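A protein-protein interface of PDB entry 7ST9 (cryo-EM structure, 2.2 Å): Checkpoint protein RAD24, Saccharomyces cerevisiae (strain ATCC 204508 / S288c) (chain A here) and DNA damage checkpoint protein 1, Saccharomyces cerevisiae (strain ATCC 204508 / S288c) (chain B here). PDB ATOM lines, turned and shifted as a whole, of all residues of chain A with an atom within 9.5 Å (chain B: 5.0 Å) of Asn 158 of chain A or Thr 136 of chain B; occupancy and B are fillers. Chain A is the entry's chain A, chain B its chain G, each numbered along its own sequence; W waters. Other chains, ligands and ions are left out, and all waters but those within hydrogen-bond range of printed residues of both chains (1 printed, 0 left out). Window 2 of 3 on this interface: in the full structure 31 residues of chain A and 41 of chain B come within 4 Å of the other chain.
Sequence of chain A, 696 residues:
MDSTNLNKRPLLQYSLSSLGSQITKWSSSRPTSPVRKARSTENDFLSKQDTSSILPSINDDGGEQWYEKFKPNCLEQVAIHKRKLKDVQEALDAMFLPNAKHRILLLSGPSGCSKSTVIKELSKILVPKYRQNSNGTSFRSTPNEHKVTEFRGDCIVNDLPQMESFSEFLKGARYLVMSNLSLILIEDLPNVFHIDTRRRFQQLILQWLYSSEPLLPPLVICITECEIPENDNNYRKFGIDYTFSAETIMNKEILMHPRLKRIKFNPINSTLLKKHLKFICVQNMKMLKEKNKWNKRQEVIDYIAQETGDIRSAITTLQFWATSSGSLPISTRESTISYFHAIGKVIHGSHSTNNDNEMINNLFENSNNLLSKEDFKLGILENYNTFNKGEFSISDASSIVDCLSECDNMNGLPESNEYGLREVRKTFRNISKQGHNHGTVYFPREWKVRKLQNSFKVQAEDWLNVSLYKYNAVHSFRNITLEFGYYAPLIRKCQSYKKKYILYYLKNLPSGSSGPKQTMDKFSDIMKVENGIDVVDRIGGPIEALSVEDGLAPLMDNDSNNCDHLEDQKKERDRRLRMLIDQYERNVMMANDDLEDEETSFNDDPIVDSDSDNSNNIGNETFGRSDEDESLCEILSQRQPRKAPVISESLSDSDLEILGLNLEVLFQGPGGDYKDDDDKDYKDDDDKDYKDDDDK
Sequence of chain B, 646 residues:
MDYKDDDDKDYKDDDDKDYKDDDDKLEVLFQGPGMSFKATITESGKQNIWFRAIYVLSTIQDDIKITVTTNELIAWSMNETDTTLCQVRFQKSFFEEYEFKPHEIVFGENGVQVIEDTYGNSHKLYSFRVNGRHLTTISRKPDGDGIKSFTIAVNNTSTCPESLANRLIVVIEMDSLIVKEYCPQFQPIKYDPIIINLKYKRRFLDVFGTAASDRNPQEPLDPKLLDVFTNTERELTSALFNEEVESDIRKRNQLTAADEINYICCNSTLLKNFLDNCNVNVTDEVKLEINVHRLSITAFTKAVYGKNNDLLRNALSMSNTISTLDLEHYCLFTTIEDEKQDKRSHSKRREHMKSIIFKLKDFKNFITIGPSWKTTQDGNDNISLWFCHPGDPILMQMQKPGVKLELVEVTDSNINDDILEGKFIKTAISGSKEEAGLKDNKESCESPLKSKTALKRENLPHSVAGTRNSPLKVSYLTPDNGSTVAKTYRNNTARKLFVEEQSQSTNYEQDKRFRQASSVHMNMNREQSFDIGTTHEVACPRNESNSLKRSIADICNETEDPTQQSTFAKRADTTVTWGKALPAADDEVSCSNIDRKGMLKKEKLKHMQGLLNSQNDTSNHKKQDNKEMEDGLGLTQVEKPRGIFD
The side-chain hydroxyl (OG) of Ser 58 of chain B lies within hydrogen-bond range of the side-chain amide nitrogen (ND2) of Asn 158 of chain A, at 2.7 Å. The backbone carbonyl oxygen of Ile 156 of chain A is in hydrogen-bond range of the guanidinium group of Arg 133 of chain B.
O of Tyr 55 of chain B lies within hydrogen-bond range of OG of Ser 58 of chain B. O of Gly 132 of chain B sits at hydrogen-bond distance from OG1 of Thr 136 of chain B (2.8 Å). OG1 of Thr 137 of chain B sits at hydrogen-bond distance from O of Arg 133 of chain B.
Among the printed residues, pairs that only touch across the chains: Val 157 of chain A with Thr 59 of chain B (3.4 Å), Asp 159 of chain A with Tyr 55 of chain B (3.7 Å), Asp 159 of chain A with Thr 59 of chain B (3.7 Å), Asn 158 of chain A with Thr 136 of chain B (3.7 Å), Val 157 of chain A with Ser 58 of chain B (3.8 Å), Asn 158 of chain A with Arg 133 of chain B (3.8 Å) and Asn 158 of chain A with Tyr 55 of chain B (3.9 Å).
Of chain B, only Tyr 55 (3.9 Å), Ser 58 (2.7 Å), Arg 133 (3.8 Å) and Thr 136 (3.7 Å) come within 4 Å of Asn 158 of chain A. Of the printed residues of chain A, Ser 58 of chain B touches Val 157 and Asn 158. No residue of chain A comes within 4 Å of Leu 135 of chain B. No residue of chain A comes within 4 Å of Thr 137 of chain B. Printed residues of chain A within 4 Å of Thr 59 of chain B: Val 157 (3.4 Å) and Asp 159 (3.7 Å). Of the printed residues of chain B, Asp 159 of chain A touches Tyr 55 (3.7 Å) and Thr 59 (3.7 Å). Printed residues of chain A within 4 Å of Arg 133 of chain B: Ile 156 (3.2 Å) and Asn 158 (3.8 Å). Of the printed residues of chain A, Tyr 55 of chain B touches Asn 158 and Asp 159. Printed residues of chain B within 4 Å of Ile 156 of chain A: Arg 133. Pro 161 of chain A touches none of the printed residues of chain B. Cys 155 of chain A touches none of the printed residues of chain B. The nearest printed residue of chain B that does not touch Val 157 of chain A is Arg 133 of chain B (4.4 Å).
Hydrophobic or aromatic side chains of chain A that line the printed part of chain B: Ile 156 and Val 157. Among the printed residues, no Asp or Glu carboxylate lies within 4 Å of a Lys or Arg side-chain nitrogen of the other chain.
Water W1 lies within hydrogen-bond range of O of Arg 133 of chain B (2.9 Å), OD1 of Asn 158 of chain A (3.1 Å) and OG1 of Thr 137 of chain B (3.1 Å).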
ATOM      1  N   CYS A 155     -14.760  -6.325   2.779  1.00  0.00           N
ATOM      2  CA  CYS A 155     -13.749  -6.848   1.871  1.00  0.00           C
ATOM      3  C   CYS A 155     -14.081  -8.284   1.484  1.00  0.00           C
ATOM      4  O   CYS A 155     -14.362  -9.122   2.346  1.00  0.00           O
ATOM      5  CB  CYS A 155     -12.368  -6.781   2.523  1.00  0.00           C
ATOM      6  SG  CYS A 155     -11.006  -7.251   1.429  1.00  0.00           S
ATOM      7  N   ILE A 156     -14.049  -8.565   0.184  1.00  0.00           N
ATOM      8  CA  ILE A 156     -14.312  -9.897  -0.346  1.00  0.00           C
ATOM      9  C   ILE A 156     -13.171 -10.258  -1.285  1.00  0.00           C
ATOM     10  O   ILE A 156     -12.874  -9.508  -2.222  1.00  0.00           O
ATOM     11  CB  ILE A 156     -15.663  -9.971  -1.080  1.00  0.00           C
ATOM     12  CG1 ILE A 156     -16.809 -10.056  -0.069  1.00  0.00           C
ATOM     13  CG2 ILE A 156     -15.696 -11.171  -2.023  1.00  0.00           C
ATOM     14  CD1 ILE A 156     -18.180  -9.836  -0.675  1.00  0.00           C
ATOM     15  N   VAL A 157     -12.537 -11.399  -1.036  1.00  0.00           N
ATOM     16  CA  VAL A 157     -11.477 -11.910  -1.893  1.00  0.00           C
ATOM     17  C   VAL A 157     -11.967 -13.192  -2.554  1.00  0.00           C
ATOM     18  O   VAL A 157     -12.946 -13.812  -2.129  1.00  0.00           O
ATOM     19  CB  VAL A 157     -10.162 -12.152  -1.124  1.00  0.00           C
ATOM     20  CG1 VAL A 157      -9.556 -10.829  -0.683  1.00  0.00           C
ATOM     21  CG2 VAL A 157     -10.396 -13.064   0.070  1.00  0.00           C
ATOM     22  N   ASN A 158     -11.265 -13.589  -3.615  1.00  0.00           N
ATOM     23  CA  ASN A 158     -11.737 -14.690  -4.448  1.00  0.00           C
ATOM     24  C   ASN A 158     -11.672 -16.024  -3.709  1.00  0.00           C
ATOM     25  O   ASN A 158     -12.639 -16.795  -3.717  1.00  0.00           O
ATOM     26  CB  ASN A 158     -10.917 -14.755  -5.737  1.00  0.00           C
ATOM     27  CG  ASN A 158     -11.772 -14.606  -6.979  1.00  0.00           C
ATOM     28  OD1 ASN A 158     -12.956 -14.934  -6.975  1.00  0.00           O
ATOM     29  ND2 ASN A 158     -11.169 -14.113  -8.054  1.00  0.00           N
ATOM     30  N   ASP A 159     -10.546 -16.311  -3.058  1.00  0.00           N
ATOM     31  CA  ASP A 159     -10.262 -17.643  -2.522  1.00  0.00           C
ATOM     32  C   ASP A 159     -10.475 -17.719  -1.016  1.00  0.00           C
ATOM     33  O   ASP A 159      -9.702 -18.370  -0.306  1.00  0.00           O
ATOM     34  CB  ASP A 159      -8.836 -18.051  -2.882  1.00  0.00           C
ATOM     35  CG  ASP A 159      -8.564 -19.523  -2.625  1.00  0.00           C
ATOM     36  OD1 ASP A 159      -9.532 -20.284  -2.414  1.00  0.00           O
ATOM     37  OD2 ASP A 159      -7.379 -19.916  -2.633  1.00  0.00           O
ATOM     38  N   LEU A 160     -11.509 -17.062  -0.495  1.00  0.00           N
ATOM     39  CA  LEU A 160     -11.750 -17.077   0.941  1.00  0.00           C
ATOM     40  C   LEU A 160     -13.243 -17.032   1.251  1.00  0.00           C
ATOM     41  O   LEU A 160     -13.941 -16.116   0.796  1.00  0.00           O
ATOM     42  CB  LEU A 160     -11.042 -15.896   1.607  1.00  0.00           C
ATOM     43  CG  LEU A 160     -10.772 -16.027   3.106  1.00  0.00           C
ATOM     44  CD1 LEU A 160      -9.720 -17.092   3.378  1.00  0.00           C
ATOM     45  CD2 LEU A 160     -10.344 -14.689   3.681  1.00  0.00           C
ATOM     46  N   PRO A 161     -13.773 -17.991   2.013  1.00  0.00           N
ATOM     47  CA  PRO A 161     -15.158 -17.867   2.480  1.00  0.00           C
ATOM     48  C   PRO A 161     -15.323 -16.654   3.384  1.00  0.00           C
ATOM     49  O   PRO A 161     -14.388 -16.224   4.061  1.00  0.00           O
ATOM     50  CB  PRO A 161     -15.401 -19.175   3.242  1.00  0.00           C
ATOM     51  CG  PRO A 161     -14.372 -20.118   2.739  1.00  0.00           C
ATOM     52  CD  PRO A 161     -13.182 -19.285   2.390  1.00  0.00           C
ATOM     53  N   GLN A 162     -16.537 -16.102   3.385  1.00  0.00           N
ATOM     54  CA  GLN A 162     -16.787 -14.863   4.117  1.00  0.00           C
ATOM     55  C   GLN A 162     -16.462 -15.018   5.599  1.00  0.00           C
ATOM     56  O   GLN A 162     -15.748 -14.191   6.178  1.00  0.00           O
ATOM     57  CB  GLN A 162     -18.241 -14.430   3.928  1.00  0.00           C
ATOM     58  CG  GLN A 162     -18.492 -12.965   4.249  1.00  0.00           C
ATOM     59  CD  GLN A 162     -17.997 -12.037   3.157  1.00  0.00           C
ATOM     60  OE1 GLN A 162     -18.385 -12.166   1.997  1.00  0.00           O
ATOM     61  NE2 GLN A 162     -17.131 -11.100   3.523  1.00  0.00           N
ATOM     62  N   PHE B  51      -4.280 -14.856 -16.715  1.00  0.00           N
ATOM     63  CA  PHE B  51      -5.433 -15.184 -15.886  1.00  0.00           C
ATOM     64  C   PHE B  51      -5.000 -15.637 -14.499  1.00  0.00           C
ATOM     65  O   PHE B  51      -5.607 -15.250 -13.497  1.00  0.00           O
ATOM     66  CB  PHE B  51      -6.278 -16.269 -16.553  1.00  0.00           C
ATOM     67  CG  PHE B  51      -7.108 -17.060 -15.584  1.00  0.00           C
ATOM     68  CD1 PHE B  51      -8.234 -16.504 -15.002  1.00  0.00           C
ATOM     69  CD2 PHE B  51      -6.752 -18.352 -15.240  1.00  0.00           C
ATOM     70  CE1 PHE B  51      -8.994 -17.225 -14.102  1.00  0.00           C
ATOM     71  CE2 PHE B  51      -7.509 -19.078 -14.341  1.00  0.00           C
ATOM     72  CZ  PHE B  51      -8.632 -18.513 -13.772  1.00  0.00           C
ATOM     73  N   ILE B  54      -3.831 -12.620 -12.434  1.00  0.00           N
ATOM     74  CA  ILE B  54      -4.967 -11.808 -12.008  1.00  0.00           C
ATOM     75  C   ILE B  54      -5.725 -12.511 -10.890  1.00  0.00           C
ATOM     76  O   ILE B  54      -6.144 -11.879  -9.913  1.00  0.00           O
ATOM     77  CB  ILE B  54      -5.876 -11.487 -13.211  1.00  0.00           C
ATOM     78  CG1 ILE B  54      -5.473 -10.154 -13.847  1.00  0.00           C
ATOM     79  CG2 ILE B  54      -7.340 -11.414 -12.795  1.00  0.00           C
ATOM     80  CD1 ILE B  54      -4.011 -10.057 -14.222  1.00  0.00           C
ATOM     81  N   TYR B  55      -5.910 -13.829 -11.008  1.00  0.00           N
ATOM     82  CA  TYR B  55      -6.629 -14.571  -9.978  1.00  0.00           C
ATOM     83  C   TYR B  55      -5.894 -14.526  -8.642  1.00  0.00           C
ATOM     84  O   TYR B  55      -6.515 -14.334  -7.590  1.00  0.00           O
ATOM     85  CB  TYR B  55      -6.833 -16.020 -10.426  1.00  0.00           C
ATOM     86  CG  TYR B  55      -7.352 -16.924  -9.335  1.00  0.00           C
ATOM     87  CD1 TYR B  55      -8.705 -16.972  -9.032  1.00  0.00           C
ATOM     88  CD2 TYR B  55      -6.488 -17.727  -8.602  1.00  0.00           C
ATOM     89  CE1 TYR B  55      -9.184 -17.794  -8.033  1.00  0.00           C
ATOM     90  CE2 TYR B  55      -6.959 -18.552  -7.600  1.00  0.00           C
ATOM     91  CZ  TYR B  55      -8.307 -18.582  -7.319  1.00  0.00           C
ATOM     92  OH  TYR B  55      -8.783 -19.402  -6.324  1.00  0.00           O
ATOM     93  N   SER B  58      -6.252 -11.174  -7.119  1.00  0.00           N
ATOM     94  CA  SER B  58      -7.604 -11.036  -6.589  1.00  0.00           C
ATOM     95  C   SER B  58      -7.761 -11.776  -5.269  1.00  0.00           C
ATOM     96  O   SER B  58      -8.512 -11.332  -4.394  1.00  0.00           O
ATOM     97  CB  SER B  58      -8.621 -11.546  -7.610  1.00  0.00           C
ATOM     98  OG  SER B  58      -8.781 -12.950  -7.516  1.00  0.00           O
ATOM     99  N   THR B  59      -7.080 -12.913  -5.110  1.00  0.00           N
ATOM    100  CA  THR B  59      -7.099 -13.590  -3.817  1.00  0.00           C
ATOM    101  C   THR B  59      -6.429 -12.745  -2.743  1.00  0.00           C
ATOM    102  O   THR B  59      -6.850 -12.776  -1.581  1.00  0.00           O
ATOM    103  CB  THR B  59      -6.413 -14.959  -3.894  1.00  0.00           C
ATOM    104  OG1 THR B  59      -4.994 -14.787  -3.998  1.00  0.00           O
ATOM    105  CG2 THR B  59      -6.920 -15.770  -5.080  1.00  0.00           C
ATOM    106  N   GLY B 132     -10.865  -6.901  -8.532  1.00  0.00           N
ATOM    107  CA  GLY B 132     -10.099  -8.077  -8.913  1.00  0.00           C
ATOM    108  C   GLY B 132     -10.967  -9.234  -9.371  1.00  0.00           C
ATOM    109  O   GLY B 132     -10.647  -9.909 -10.353  1.00  0.00           O
ATOM    110  N   ARG B 133     -12.069  -9.487  -8.663  1.00  0.00           N
ATOM    111  CA  ARG B 133     -12.930 -10.610  -9.021  1.00  0.00           C
ATOM    112  C   ARG B 133     -13.514 -10.431 -10.417  1.00  0.00           C
ATOM    113  O   ARG B 133     -13.585 -11.389 -11.197  1.00  0.00           O
ATOM    114  CB  ARG B 133     -14.047 -10.765  -7.990  1.00  0.00           C
ATOM    115  CG  ARG B 133     -13.557 -11.191  -6.617  1.00  0.00           C
ATOM    116  CD  ARG B 133     -14.685 -11.732  -5.754  1.00  0.00           C
ATOM    117  NE  ARG B 133     -15.883 -10.902  -5.812  1.00  0.00           N
ATOM    118  CZ  ARG B 133     -15.986  -9.690  -5.282  1.00  0.00           C
ATOM    119  NH1 ARG B 133     -14.972  -9.122  -4.651  1.00  0.00           N
ATOM    120  NH2 ARG B 133     -17.136  -9.031  -5.393  1.00  0.00           N
ATOM    121  N   HIS B 134     -13.940  -9.211 -10.749  1.00  0.00           N
ATOM    122  CA  HIS B 134     -14.506  -8.956 -12.069  1.00  0.00           C
ATOM    123  C   HIS B 134     -13.472  -9.203 -13.162  1.00  0.00           C
ATOM    124  O   HIS B 134     -13.764  -9.843 -14.180  1.00  0.00           O
ATOM    125  CB  HIS B 134     -15.035  -7.523 -12.135  1.00  0.00           C
ATOM    126  CG  HIS B 134     -16.214  -7.275 -11.248  1.00  0.00           C
ATOM    127  ND1 HIS B 134     -16.745  -6.020 -11.047  1.00  0.00           N
ATOM    128  CD2 HIS B 134     -16.964  -8.123 -10.504  1.00  0.00           C
ATOM    129  CE1 HIS B 134     -17.771  -6.104 -10.219  1.00  0.00           C
ATOM    130  NE2 HIS B 134     -17.925  -7.370  -9.876  1.00  0.00           N
ATOM    131  N   LEU B 135     -12.248  -8.709 -12.961  1.00  0.00           N
ATOM    132  CA  LEU B 135     -11.202  -8.911 -13.957  1.00  0.00           C
ATOM    133  C   LEU B 135     -10.864 -10.388 -14.104  1.00  0.00           C
ATOM    134  O   LEU B 135     -10.635 -10.872 -15.220  1.00  0.00           O
ATOM    135  CB  LEU B 135      -9.958  -8.105 -13.580  1.00  0.00           C
ATOM    136  CG  LEU B 135      -8.902  -7.912 -14.672  1.00  0.00           C
ATOM    137  CD1 LEU B 135      -9.497  -7.278 -15.923  1.00  0.00           C
ATOM    138  CD2 LEU B 135      -7.746  -7.072 -14.150  1.00  0.00           C
ATOM    139  N   THR B 136     -10.826 -11.124 -12.990  1.00  0.00           N
ATOM    140  CA  THR B 136     -10.566 -12.558 -13.066  1.00  0.00           C
ATOM    141  C   THR B 136     -11.665 -13.274 -13.841  1.00  0.00           C
ATOM    142  O   THR B 136     -11.382 -14.139 -14.677  1.00  0.00           O
ATOM    143  CB  THR B 136     -10.438 -13.147 -11.660  1.00  0.00           C
ATOM    144  OG1 THR B 136      -9.463 -12.410 -10.913  1.00  0.00           O
ATOM    145  CG2 THR B 136     -10.020 -14.610 -11.730  1.00  0.00           C
ATOM    146  N   THR B 137     -12.924 -12.921 -13.581  1.00  0.00           N
ATOM    147  CA  THR B 137     -14.027 -13.532 -14.316  1.00  0.00           C
ATOM    148  C   THR B 137     -13.941 -13.213 -15.803  1.00  0.00           C
ATOM    149  O   THR B 137     -14.284 -14.049 -16.646  1.00  0.00           O
ATOM    150  CB  THR B 137     -15.365 -13.060 -13.747  1.00  0.00           C
ATOM    151  OG1 THR B 137     -15.482 -13.474 -12.380  1.00  0.00           O
ATOM    152  CG2 THR B 137     -16.524 -13.638 -14.548  1.00  0.00           C
ATOM    153  N   ILE B 138     -13.498 -12.002 -16.145  1.00  0.00           N
ATOM    154  CA  ILE B 138     -13.395 -11.625 -17.551  1.00  0.00           C
ATOM    155  C   ILE B 138     -12.283 -12.406 -18.243  1.00  0.00           C
ATOM    156  O   ILE B 138     -12.407 -12.777 -19.417  1.00  0.00           O
ATOM    157  CB  ILE B 138     -13.180 -10.106 -17.681  1.00  0.00           C
ATOM    158  CG1 ILE B 138     -14.495  -9.360 -17.452  1.00  0.00           C
ATOM    159  CG2 ILE B 138     -12.615  -9.762 -19.053  1.00  0.00           C
ATOM    160  CD1 ILE B 138     -14.315  -7.893 -17.122  1.00  0.00           C
ATOM    161  N   SER B 139     -11.182 -12.661 -17.540  1.00  0.00           N
ATOM    162  CA  SER B 139      -9.955 -13.142 -18.165  1.00  0.00           C
ATOM    163  C   SER B 139      -9.832 -14.662 -18.203  1.00  0.00           C
ATOM    164  O   SER B 139      -8.810 -15.165 -18.680  1.00  0.00           O
ATOM    165  CB  SER B 139      -8.740 -12.560 -17.434  1.00  0.00           C
ATOM    166  OG  SER B 139      -8.861 -11.158 -17.277  1.00  0.00           O
ATOM    167  N   ARG B 140     -10.826 -15.405 -17.730  1.00  0.00           N
ATOM    168  CA  ARG B 140     -10.720 -16.857 -17.684  1.00  0.00           C
ATOM    169  C   ARG B 140     -11.122 -17.472 -19.021  1.00  0.00           C
ATOM    170  O   ARG B 140     -11.967 -16.943 -19.746  1.00  0.00           O
ATOM    171  CB  ARG B 140     -11.579 -17.452 -16.561  1.00  0.00           C
ATOM    172  CG  ARG B 140     -12.976 -16.871 -16.409  1.00  0.00           C
ATOM    173  CD  ARG B 140     -13.877 -17.273 -17.559  1.00  0.00           C
ATOM    174  NE  ARG B 140     -15.255 -17.478 -17.132  1.00  0.00           N
ATOM    175  CZ  ARG B 140     -16.149 -18.185 -17.809  1.00  0.00           C
ATOM    176  NH1 ARG B 140     -15.844 -18.773 -18.955  1.00  0.00           N
ATOM    177  NH2 ARG B 140     -17.381 -18.305 -17.325  1.00  0.00           N
HETATM  178  O   HOH W   1     -13.842 -13.905  -9.767  1.00  0.00           O
